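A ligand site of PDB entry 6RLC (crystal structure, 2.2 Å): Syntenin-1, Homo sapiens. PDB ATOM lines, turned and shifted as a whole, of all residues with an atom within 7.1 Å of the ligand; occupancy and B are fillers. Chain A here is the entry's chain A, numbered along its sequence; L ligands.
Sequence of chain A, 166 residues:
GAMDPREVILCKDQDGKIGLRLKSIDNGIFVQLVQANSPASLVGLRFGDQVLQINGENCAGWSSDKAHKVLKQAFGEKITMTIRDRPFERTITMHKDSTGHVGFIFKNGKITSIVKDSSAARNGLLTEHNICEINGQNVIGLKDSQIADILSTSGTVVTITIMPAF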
ATOM      1  N   LYS A  96       6.621  15.734 -11.903  1.00  0.00           N
ATOM      2  CA  LYS A  96       5.145  15.942 -11.983  1.00  0.00           C
ATOM      3  C   LYS A  96       4.551  14.916 -12.952  1.00  0.00           C
ATOM      4  O   LYS A  96       5.166  14.635 -13.983  1.00  0.00           O
ATOM      5  CB  LYS A  96       4.823  17.366 -12.427  1.00  0.00           C
ATOM      6  CG  LYS A  96       5.214  18.460 -11.427  1.00  0.00           C
ATOM      7  CD  LYS A  96       4.785  19.841 -11.872  1.00  0.00           C
ATOM      8  CE  LYS A  96       4.748  20.861 -10.763  1.00  0.00           C
ATOM      9  NZ  LYS A  96       4.297  22.192 -11.254  1.00  0.00           N
ATOM     10  N   ASP A  97       3.391  14.368 -12.606  1.00  0.00           N
ATOM     11  CA  ASP A  97       2.583  13.462 -13.474  1.00  0.00           C
ATOM     12  C   ASP A  97       1.766  14.320 -14.450  1.00  0.00           C
ATOM     13  O   ASP A  97       1.908  15.574 -14.409  1.00  0.00           O
ATOM     14  CB  ASP A  97       1.733  12.518 -12.620  1.00  0.00           C
ATOM     15  CG  ASP A  97       0.604  13.186 -11.860  1.00  0.00           C
ATOM     16  OD1 ASP A  97       0.236  14.328 -12.193  1.00  0.00           O
ATOM     17  OD2 ASP A  97       0.076  12.553 -10.942  1.00  0.00           O
ATOM     18  N   THR A  99      -1.229  15.233 -14.360  1.00  0.00           N
ATOM     19  CA  THR A  99      -2.099  16.198 -13.618  1.00  0.00           C
ATOM     20  C   THR A  99      -1.273  17.314 -12.944  1.00  0.00           C
ATOM     21  O   THR A  99      -1.899  18.127 -12.247  1.00  0.00           O
ATOM     22  CB  THR A  99      -2.943  15.472 -12.564  1.00  0.00           C
ATOM     23  OG1 THR A  99      -2.075  15.003 -11.516  1.00  0.00           O
ATOM     24  CG2 THR A  99      -3.710  14.295 -13.126  1.00  0.00           C
ATOM     25  N   GLY A 100       0.061  17.331 -13.107  1.00  0.00           N
ATOM     26  CA  GLY A 100       0.952  18.347 -12.483  1.00  0.00           C
ATOM     27  C   GLY A 100       1.269  18.071 -11.021  1.00  0.00           C
ATOM     28  O   GLY A 100       1.763  19.010 -10.358  1.00  0.00           O
ATOM     29  N   HIS A 101       1.016  16.852 -10.518  1.00  0.00           N
ATOM     30  CA  HIS A 101       1.255  16.454  -9.098  1.00  0.00           C
ATOM     31  C   HIS A 101       2.502  15.573  -8.970  1.00  0.00           C
ATOM     32  O   HIS A 101       2.761  14.757  -9.875  1.00  0.00           O
ATOM     33  CB  HIS A 101       0.027  15.753  -8.512  1.00  0.00           C
ATOM     34  CG  HIS A 101      -1.163  16.645  -8.434  1.00  0.00           C
ATOM     35  ND1 HIS A 101      -2.132  16.682  -9.422  1.00  0.00           N
ATOM     36  CD2 HIS A 101      -1.517  17.576  -7.537  1.00  0.00           C
ATOM     37  CE1 HIS A 101      -3.036  17.587  -9.116  1.00  0.00           C
ATOM     38  NE2 HIS A 101      -2.691  18.139  -7.959  1.00  0.00           N
ATOM     39  N   VAL A 102       3.237  15.717  -7.863  1.00  0.00           N
ATOM     40  CA  VAL A 102       4.379  14.832  -7.481  1.00  0.00           C
ATOM     41  C   VAL A 102       3.898  13.740  -6.514  1.00  0.00           C
ATOM     42  O   VAL A 102       4.530  12.676  -6.488  1.00  0.00           O
ATOM     43  CB  VAL A 102       5.563  15.643  -6.919  1.00  0.00           C
ATOM     44  CG1 VAL A 102       6.183  16.476  -8.015  1.00  0.00           C
ATOM     45  CG2 VAL A 102       5.180  16.516  -5.742  1.00  0.00           C
ATOM     46  N   GLY A 103       2.847  14.004  -5.736  1.00  0.00           N
ATOM     47  CA  GLY A 103       2.116  12.980  -4.960  1.00  0.00           C
ATOM     48  C   GLY A 103       2.370  13.033  -3.454  1.00  0.00           C
ATOM     49  O   GLY A 103       2.644  11.989  -2.883  1.00  0.00           O
ATOM     50  N   PHE A 104       2.180  14.175  -2.803  1.00  0.00           N
ATOM     51  CA  PHE A 104       2.161  14.239  -1.316  1.00  0.00           C
ATOM     52  C   PHE A 104       1.195  15.309  -0.832  1.00  0.00           C
ATOM     53  O   PHE A 104       0.918  16.287  -1.531  1.00  0.00           O
ATOM     54  CB  PHE A 104       3.551  14.425  -0.697  1.00  0.00           C
ATOM     55  CG  PHE A 104       4.258  15.719  -1.006  1.00  0.00           C
ATOM     56  CD1 PHE A 104       4.133  16.812  -0.178  1.00  0.00           C
ATOM     57  CD2 PHE A 104       5.134  15.813  -2.053  1.00  0.00           C
ATOM     58  CE1 PHE A 104       4.812  17.992  -0.447  1.00  0.00           C
ATOM     59  CE2 PHE A 104       5.822  16.978  -2.315  1.00  0.00           C
ATOM     60  CZ  PHE A 104       5.629  18.085  -1.527  1.00  0.00           C
ATOM     61  N   ILE A 105       0.727  15.077   0.401  1.00  0.00           N
ATOM     62  CA  ILE A 105      -0.052  16.035   1.223  1.00  0.00           C
ATOM     63  C   ILE A 105       0.878  16.594   2.294  1.00  0.00           C
ATOM     64  O   ILE A 105       1.731  15.832   2.800  1.00  0.00           O
ATOM     65  CB  ILE A 105      -1.301  15.360   1.834  1.00  0.00           C
ATOM     66  CG1 ILE A 105      -2.121  16.346   2.661  1.00  0.00           C
ATOM     67  CG2 ILE A 105      -0.977  14.148   2.649  1.00  0.00           C
ATOM     68  CD1 ILE A 105      -2.667  17.457   1.848  1.00  0.00           C
ATOM     69  N   PHE A 106       0.719  17.857   2.633  1.00  0.00           N
ATOM     70  CA  PHE A 106       1.456  18.495   3.748  1.00  0.00           C
ATOM     71  C   PHE A 106       0.525  19.451   4.499  1.00  0.00           C
ATOM     72  O   PHE A 106      -0.543  19.853   3.958  1.00  0.00           O
ATOM     73  CB  PHE A 106       2.682  19.217   3.207  1.00  0.00           C
ATOM     74  CG  PHE A 106       2.385  20.403   2.330  1.00  0.00           C
ATOM     75  CD1 PHE A 106       2.049  20.229   0.995  1.00  0.00           C
ATOM     76  CD2 PHE A 106       2.413  21.703   2.841  1.00  0.00           C
ATOM     77  CE1 PHE A 106       1.778  21.339   0.191  1.00  0.00           C
ATOM     78  CE2 PHE A 106       2.179  22.806   2.031  1.00  0.00           C
ATOM     79  CZ  PHE A 106       1.858  22.624   0.709  1.00  0.00           C
ATOM     80  N   LYS A 107       0.906  19.761   5.742  1.00  0.00           N
ATOM     81  CA  LYS A 107       0.215  20.742   6.601  1.00  0.00           C
ATOM     82  C   LYS A 107       1.278  21.416   7.480  1.00  0.00           C
ATOM     83  O   LYS A 107       2.127  20.681   8.044  1.00  0.00           O
ATOM     84  CB  LYS A 107      -0.868  20.090   7.462  1.00  0.00           C
ATOM     85  CG  LYS A 107      -1.763  21.105   8.157  1.00  0.00           C
ATOM     86  CD  LYS A 107      -2.638  20.573   9.253  1.00  0.00           C
ATOM     87  CE  LYS A 107      -3.587  21.645   9.771  1.00  0.00           C
ATOM     88  NZ  LYS A 107      -4.759  21.073  10.493  1.00  0.00           N
ATOM     89  N   ASN A 108       1.222  22.743   7.559  1.00  0.00           N
ATOM     90  CA  ASN A 108       2.195  23.593   8.285  1.00  0.00           C
ATOM     91  C   ASN A 108       3.614  23.254   7.792  1.00  0.00           C
ATOM     92  O   ASN A 108       4.510  23.142   8.620  1.00  0.00           O
ATOM     93  CB  ASN A 108       2.087  23.409   9.800  1.00  0.00           C
ATOM     94  CG  ASN A 108       0.695  23.441  10.417  1.00  0.00           C
ATOM     95  OD1 ASN A 108      -0.283  24.045   9.959  1.00  0.00           O
ATOM     96  ND2 ASN A 108       0.629  22.806  11.569  1.00  0.00           N
ATOM     97  N   VAL A 115       1.121   9.882  -1.781  1.00  0.00           N
ATOM     98  CA  VAL A 115       0.077   9.325  -2.680  1.00  0.00           C
ATOM     99  C   VAL A 115       0.645   8.072  -3.361  1.00  0.00           C
ATOM    100  O   VAL A 115       1.760   8.113  -3.893  1.00  0.00           O
ATOM    101  CB  VAL A 115      -0.418  10.387  -3.680  1.00  0.00           C
ATOM    102  CG1 VAL A 115      -1.456   9.840  -4.644  1.00  0.00           C
ATOM    103  CG2 VAL A 115      -0.961  11.603  -2.950  1.00  0.00           C
ATOM    104  N   SER A 118       2.769   7.497  -7.093  1.00  0.00           N
ATOM    105  CA  SER A 118       3.230   8.867  -7.427  1.00  0.00           C
ATOM    106  C   SER A 118       4.757   8.873  -7.522  1.00  0.00           C
ATOM    107  O   SER A 118       5.410   7.931  -7.048  1.00  0.00           O
ATOM    108  CB  SER A 118       2.770   9.841  -6.388  1.00  0.00           C
ATOM    109  OG  SER A 118       3.466   9.623  -5.161  1.00  0.00           O
ATOM    110  N   ALA A 120       6.544  10.822  -5.702  1.00  0.00           N
ATOM    111  CA  ALA A 120       6.886  10.886  -4.261  1.00  0.00           C
ATOM    112  C   ALA A 120       7.056   9.448  -3.730  1.00  0.00           C
ATOM    113  O   ALA A 120       8.054   9.193  -3.036  1.00  0.00           O
ATOM    114  CB  ALA A 120       5.852  11.659  -3.488  1.00  0.00           C
ATOM    115  N   ILE A 131       9.352  20.622   4.854  1.00  0.00           N
ATOM    116  CA  ILE A 131       9.843  21.110   3.540  1.00  0.00           C
ATOM    117  C   ILE A 131      10.687  22.360   3.818  1.00  0.00           C
ATOM    118  O   ILE A 131      10.135  23.314   4.396  1.00  0.00           O
ATOM    119  CB  ILE A 131       8.661  21.411   2.604  1.00  0.00           C
ATOM    120  CG1 ILE A 131       7.686  20.220   2.534  1.00  0.00           C
ATOM    121  CG2 ILE A 131       9.166  21.815   1.233  1.00  0.00           C
ATOM    122  CD1 ILE A 131       6.359  20.533   1.884  1.00  0.00           C
ATOM    123  N   LYS A 143       3.359  30.363   4.250  1.00  0.00           N
ATOM    124  CA  LYS A 143       2.041  29.693   4.471  1.00  0.00           C
ATOM    125  C   LYS A 143       1.930  28.522   3.503  1.00  0.00           C
ATOM    126  O   LYS A 143       2.586  28.570   2.435  1.00  0.00           O
ATOM    127  CB  LYS A 143       0.894  30.701   4.264  1.00  0.00           C
ATOM    128  CG  LYS A 143       0.995  31.981   5.080  1.00  0.00           C
ATOM    129  CD  LYS A 143       0.992  31.733   6.591  1.00  0.00           C
ATOM    130  CE  LYS A 143       2.353  31.515   7.233  1.00  0.00           C
ATOM    131  NZ  LYS A 143       2.734  32.676   8.074  1.00  0.00           N
ATOM    132  N   ASP A 144       1.142  27.507   3.857  1.00  0.00           N
ATOM    133  CA  ASP A 144       0.885  26.304   3.008  1.00  0.00           C
ATOM    134  C   ASP A 144       0.452  26.723   1.593  1.00  0.00           C
ATOM    135  O   ASP A 144       0.946  26.078   0.654  1.00  0.00           O
ATOM    136  CB  ASP A 144      -0.130  25.382   3.679  1.00  0.00           C
ATOM    137  CG  ASP A 144       0.450  24.653   4.879  1.00  0.00           C
ATOM    138  OD1 ASP A 144       1.696  24.626   4.996  1.00  0.00           O
ATOM    139  OD2 ASP A 144      -0.333  24.100   5.661  1.00  0.00           O
ATOM    140  N   SER A 145      -0.386  27.759   1.436  1.00  0.00           N
ATOM    141  CA  SER A 145      -0.899  28.172   0.110  1.00  0.00           C
ATOM    142  C   SER A 145       0.256  28.687  -0.755  1.00  0.00           C
ATOM    143  O   SER A 145       0.237  28.438  -1.976  1.00  0.00           O
ATOM    144  CB  SER A 145      -2.063  29.159   0.216  1.00  0.00           C
ATOM    145  OG  SER A 145      -1.645  30.490   0.527  1.00  0.00           O
ATOM    146  N   GLN A 146       1.254  29.318  -0.139  1.00  0.00           N
ATOM    147  CA  GLN A 146       2.441  29.867  -0.850  1.00  0.00           C
ATOM    148  C   GLN A 146       3.346  28.715  -1.267  1.00  0.00           C
ATOM    149  O   GLN A 146       3.945  28.786  -2.345  1.00  0.00           O
ATOM    150  CB  GLN A 146       3.191  30.871   0.031  1.00  0.00           C
ATOM    151  CG  GLN A 146       2.353  32.084   0.382  1.00  0.00           C
ATOM    152  CD  GLN A 146       3.118  33.037   1.270  1.00  0.00           C
ATOM    153  OE1 GLN A 146       3.418  32.757   2.438  1.00  0.00           O
ATOM    154  NE2 GLN A 146       3.493  34.153   0.690  1.00  0.00           N
ATOM    155  N   ILE A 147       3.457  27.681  -0.443  1.00  0.00           N
ATOM    156  CA  ILE A 147       4.236  26.455  -0.798  1.00  0.00           C
ATOM    157  C   ILE A 147       3.570  25.798  -2.016  1.00  0.00           C
ATOM    158  O   ILE A 147       4.283  25.525  -3.002  1.00  0.00           O
ATOM    159  CB  ILE A 147       4.385  25.524   0.414  1.00  0.00           C
ATOM    160  CG1 ILE A 147       5.196  26.228   1.516  1.00  0.00           C
ATOM    161  CG2 ILE A 147       4.994  24.192   0.010  1.00  0.00           C
ATOM    162  CD1 ILE A 147       5.387  25.412   2.776  1.00  0.00           C
ATOM    163  N   ALA A 148       2.242  25.621  -1.975  1.00  0.00           N
ATOM    164  CA  ALA A 148       1.444  25.110  -3.119  1.00  0.00           C
ATOM    165  C   ALA A 148       1.668  25.994  -4.357  1.00  0.00           C
ATOM    166  O   ALA A 148       1.852  25.412  -5.420  1.00  0.00           O
ATOM    167  CB  ALA A 148      -0.028  25.054  -2.758  1.00  0.00           C
ATOM    168  N   ASP A 149       1.689  27.325  -4.213  1.00  0.00           N
ATOM    169  CA  ASP A 149       1.912  28.263  -5.342  1.00  0.00           C
ATOM    170  C   ASP A 149       3.244  27.929  -5.998  1.00  0.00           C
ATOM    171  O   ASP A 149       3.310  27.910  -7.225  1.00  0.00           O
ATOM    172  CB  ASP A 149       1.910  29.743  -4.922  1.00  0.00           C
ATOM    173  CG  ASP A 149       0.540  30.264  -4.538  1.00  0.00           C
ATOM    174  OD1 ASP A 149      -0.473  29.673  -5.004  1.00  0.00           O
ATOM    175  OD2 ASP A 149       0.498  31.242  -3.760  1.00  0.00           O
ATOM    176  N   LEU A 151       5.028  25.097  -5.852  1.00  0.00           N
ATOM    177  CA  LEU A 151       4.959  23.742  -6.472  1.00  0.00           C
ATOM    178  C   LEU A 151       4.163  23.844  -7.779  1.00  0.00           C
ATOM    179  O   LEU A 151       4.628  23.280  -8.777  1.00  0.00           O
ATOM    180  CB  LEU A 151       4.345  22.736  -5.499  1.00  0.00           C
ATOM    181  CG  LEU A 151       5.278  22.364  -4.340  1.00  0.00           C
ATOM    182  CD1 LEU A 151       4.484  21.845  -3.142  1.00  0.00           C
ATOM    183  CD2 LEU A 151       6.291  21.331  -4.784  1.00  0.00           C
ATOM    184  N   SER A 152       3.062  24.587  -7.804  1.00  0.00           N
ATOM    185  CA  SER A 152       2.180  24.720  -8.992  1.00  0.00           C
ATOM    186  C   SER A 152       2.899  25.438 -10.134  1.00  0.00           C
ATOM    187  O   SER A 152       2.613  25.134 -11.279  1.00  0.00           O
ATOM    188  CB  SER A 152       0.899  25.363  -8.656  1.00  0.00           C
ATOM    189  OG  SER A 152      -0.108  24.351  -8.586  1.00  0.00           O
ATOM    190  N   VAL A 158      10.866  18.597  -9.819  1.00  0.00           N
ATOM    191  CA  VAL A 158      10.673  19.199  -8.473  1.00  0.00           C
ATOM    192  C   VAL A 158      11.695  18.560  -7.525  1.00  0.00           C
ATOM    193  O   VAL A 158      11.543  17.373  -7.217  1.00  0.00           O
ATOM    194  CB  VAL A 158       9.235  18.992  -7.970  1.00  0.00           C
ATOM    195  CG1 VAL A 158       9.021  19.565  -6.578  1.00  0.00           C
ATOM    196  CG2 VAL A 158       8.208  19.569  -8.933  1.00  0.00           C
HETATM  197  C1  LIG L   1       1.396  17.506  -5.503  1.00  0.00           C
HETATM  198  C2  LIG L   1      -2.229  23.664   0.685  1.00  0.00           C
HETATM  199  C3  LIG L   1      -2.106  23.318  -0.650  1.00  0.00           C
HETATM  200  C4  LIG L   1      -1.753  22.019  -0.996  1.00  0.00           C
HETATM  201  C5  LIG L   1      -1.530  21.079   0.002  1.00  0.00           C
HETATM  202  C6  LIG L   1      -2.544  18.645  -1.249  1.00  0.00           C
HETATM  203  C7  LIG L   1      -2.025  22.715   1.691  1.00  0.00           C
HETATM  204  C8  LIG L   1      -1.412  18.321  -3.404  1.00  0.00           C
HETATM  205  N1  LIG L   1      -0.066  17.942  -3.732  1.00  0.00           N
HETATM  206  C9  LIG L   1       0.781  20.914  -3.790  1.00  0.00           C
HETATM  207  O1  LIG L   1      -1.949  19.192  -4.014  1.00  0.00           O
HETATM  208 CL1  LIG L   1      -2.675  25.320   1.121  1.00  0.00          CL
HETATM  209  C10 LIG L   1       1.575  19.704  -4.287  1.00  0.00           C
HETATM  210  O2  LIG L   1       1.247  16.359  -5.041  1.00  0.00           O
HETATM  211  C11 LIG L   1       2.543  19.195  -3.214  1.00  0.00           C
HETATM  212  O3  LIG L   1       2.130  17.734  -6.489  1.00  0.00           O
HETATM  213  C12 LIG L   1       0.644  18.613  -4.804  1.00  0.00           C
HETATM  214  C13 LIG L   1      -2.144  17.621  -2.287  1.00  0.00           C
HETATM  215  C14 LIG L   1      -1.675  21.420   1.328  1.00  0.00           C
HETATM  216  S1  LIG L   1      -1.070  19.383  -0.455  1.00  0.00           S
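An oxygen (O3) of the ligand is in hydrogen-bond range of the backbone NH of Val 102 (2.7 Å). N of Phe 104 sits at hydrogen-bond distance from O2 of the ligand (3.3 Å). A nitrogen (N1) of the ligand lies within hydrogen-bond range of the backbone carbonyl oxygen of Phe 104 (2.9 Å). O2 of the ligand lies within hydrogen-bond range of N of Gly 103 (2.9 Å).
The backbone NH (N) of Ala 120 sits at hydrogen-bond distance from the backbone carbonyl oxygen (O) of Val 102, at 2.8 Å. The backbone carbonyl oxygen of Val 102 sits close to the side-chain hydroxyl of Ser 118 (3.5 Å). O of Gly 103 lies within hydrogen-bond range of N of Val 115 (2.8 Å). O of Gly 103 lies within hydrogen-bond range of OG of Ser 118 (3.4 Å). The side-chain carboxylate of Asp 97 lies within hydrogen-bond range of the backbone NH of His 101. ND1 of His 101 is in hydrogen-bond range of OG1 of Thr 99 (2.7 Å). O of Leu 151 is in hydrogen-bond range of NZ of Lys 96 (2.7 Å). OD2 of Asp 144 is in hydrogen-bond range of N of Asn 108.
His 101 touches the ligand (CA to O3, 3.0 Å). Ile 105 touches the ligand (CD1 to C6, 3.3 Å). Phe 106 touches the ligand (O to C14, 3.3 Å). Asp 144 touches the ligand (C to CL1, 3.5 Å). N of Ser 145 touches CL1 of the ligand, at 3.4 Å. Ala 148 touches the ligand (CB to C3, 3.4 Å). Leu 151 touches the ligand (CD1 to C11, 3.3 Å). Within 4 Å of the ligand: His 101, Val 102, Gly 103, Phe 104, Ile 105, Phe 106, Asp 144, Ser 145, Ala 148 and Leu 151.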
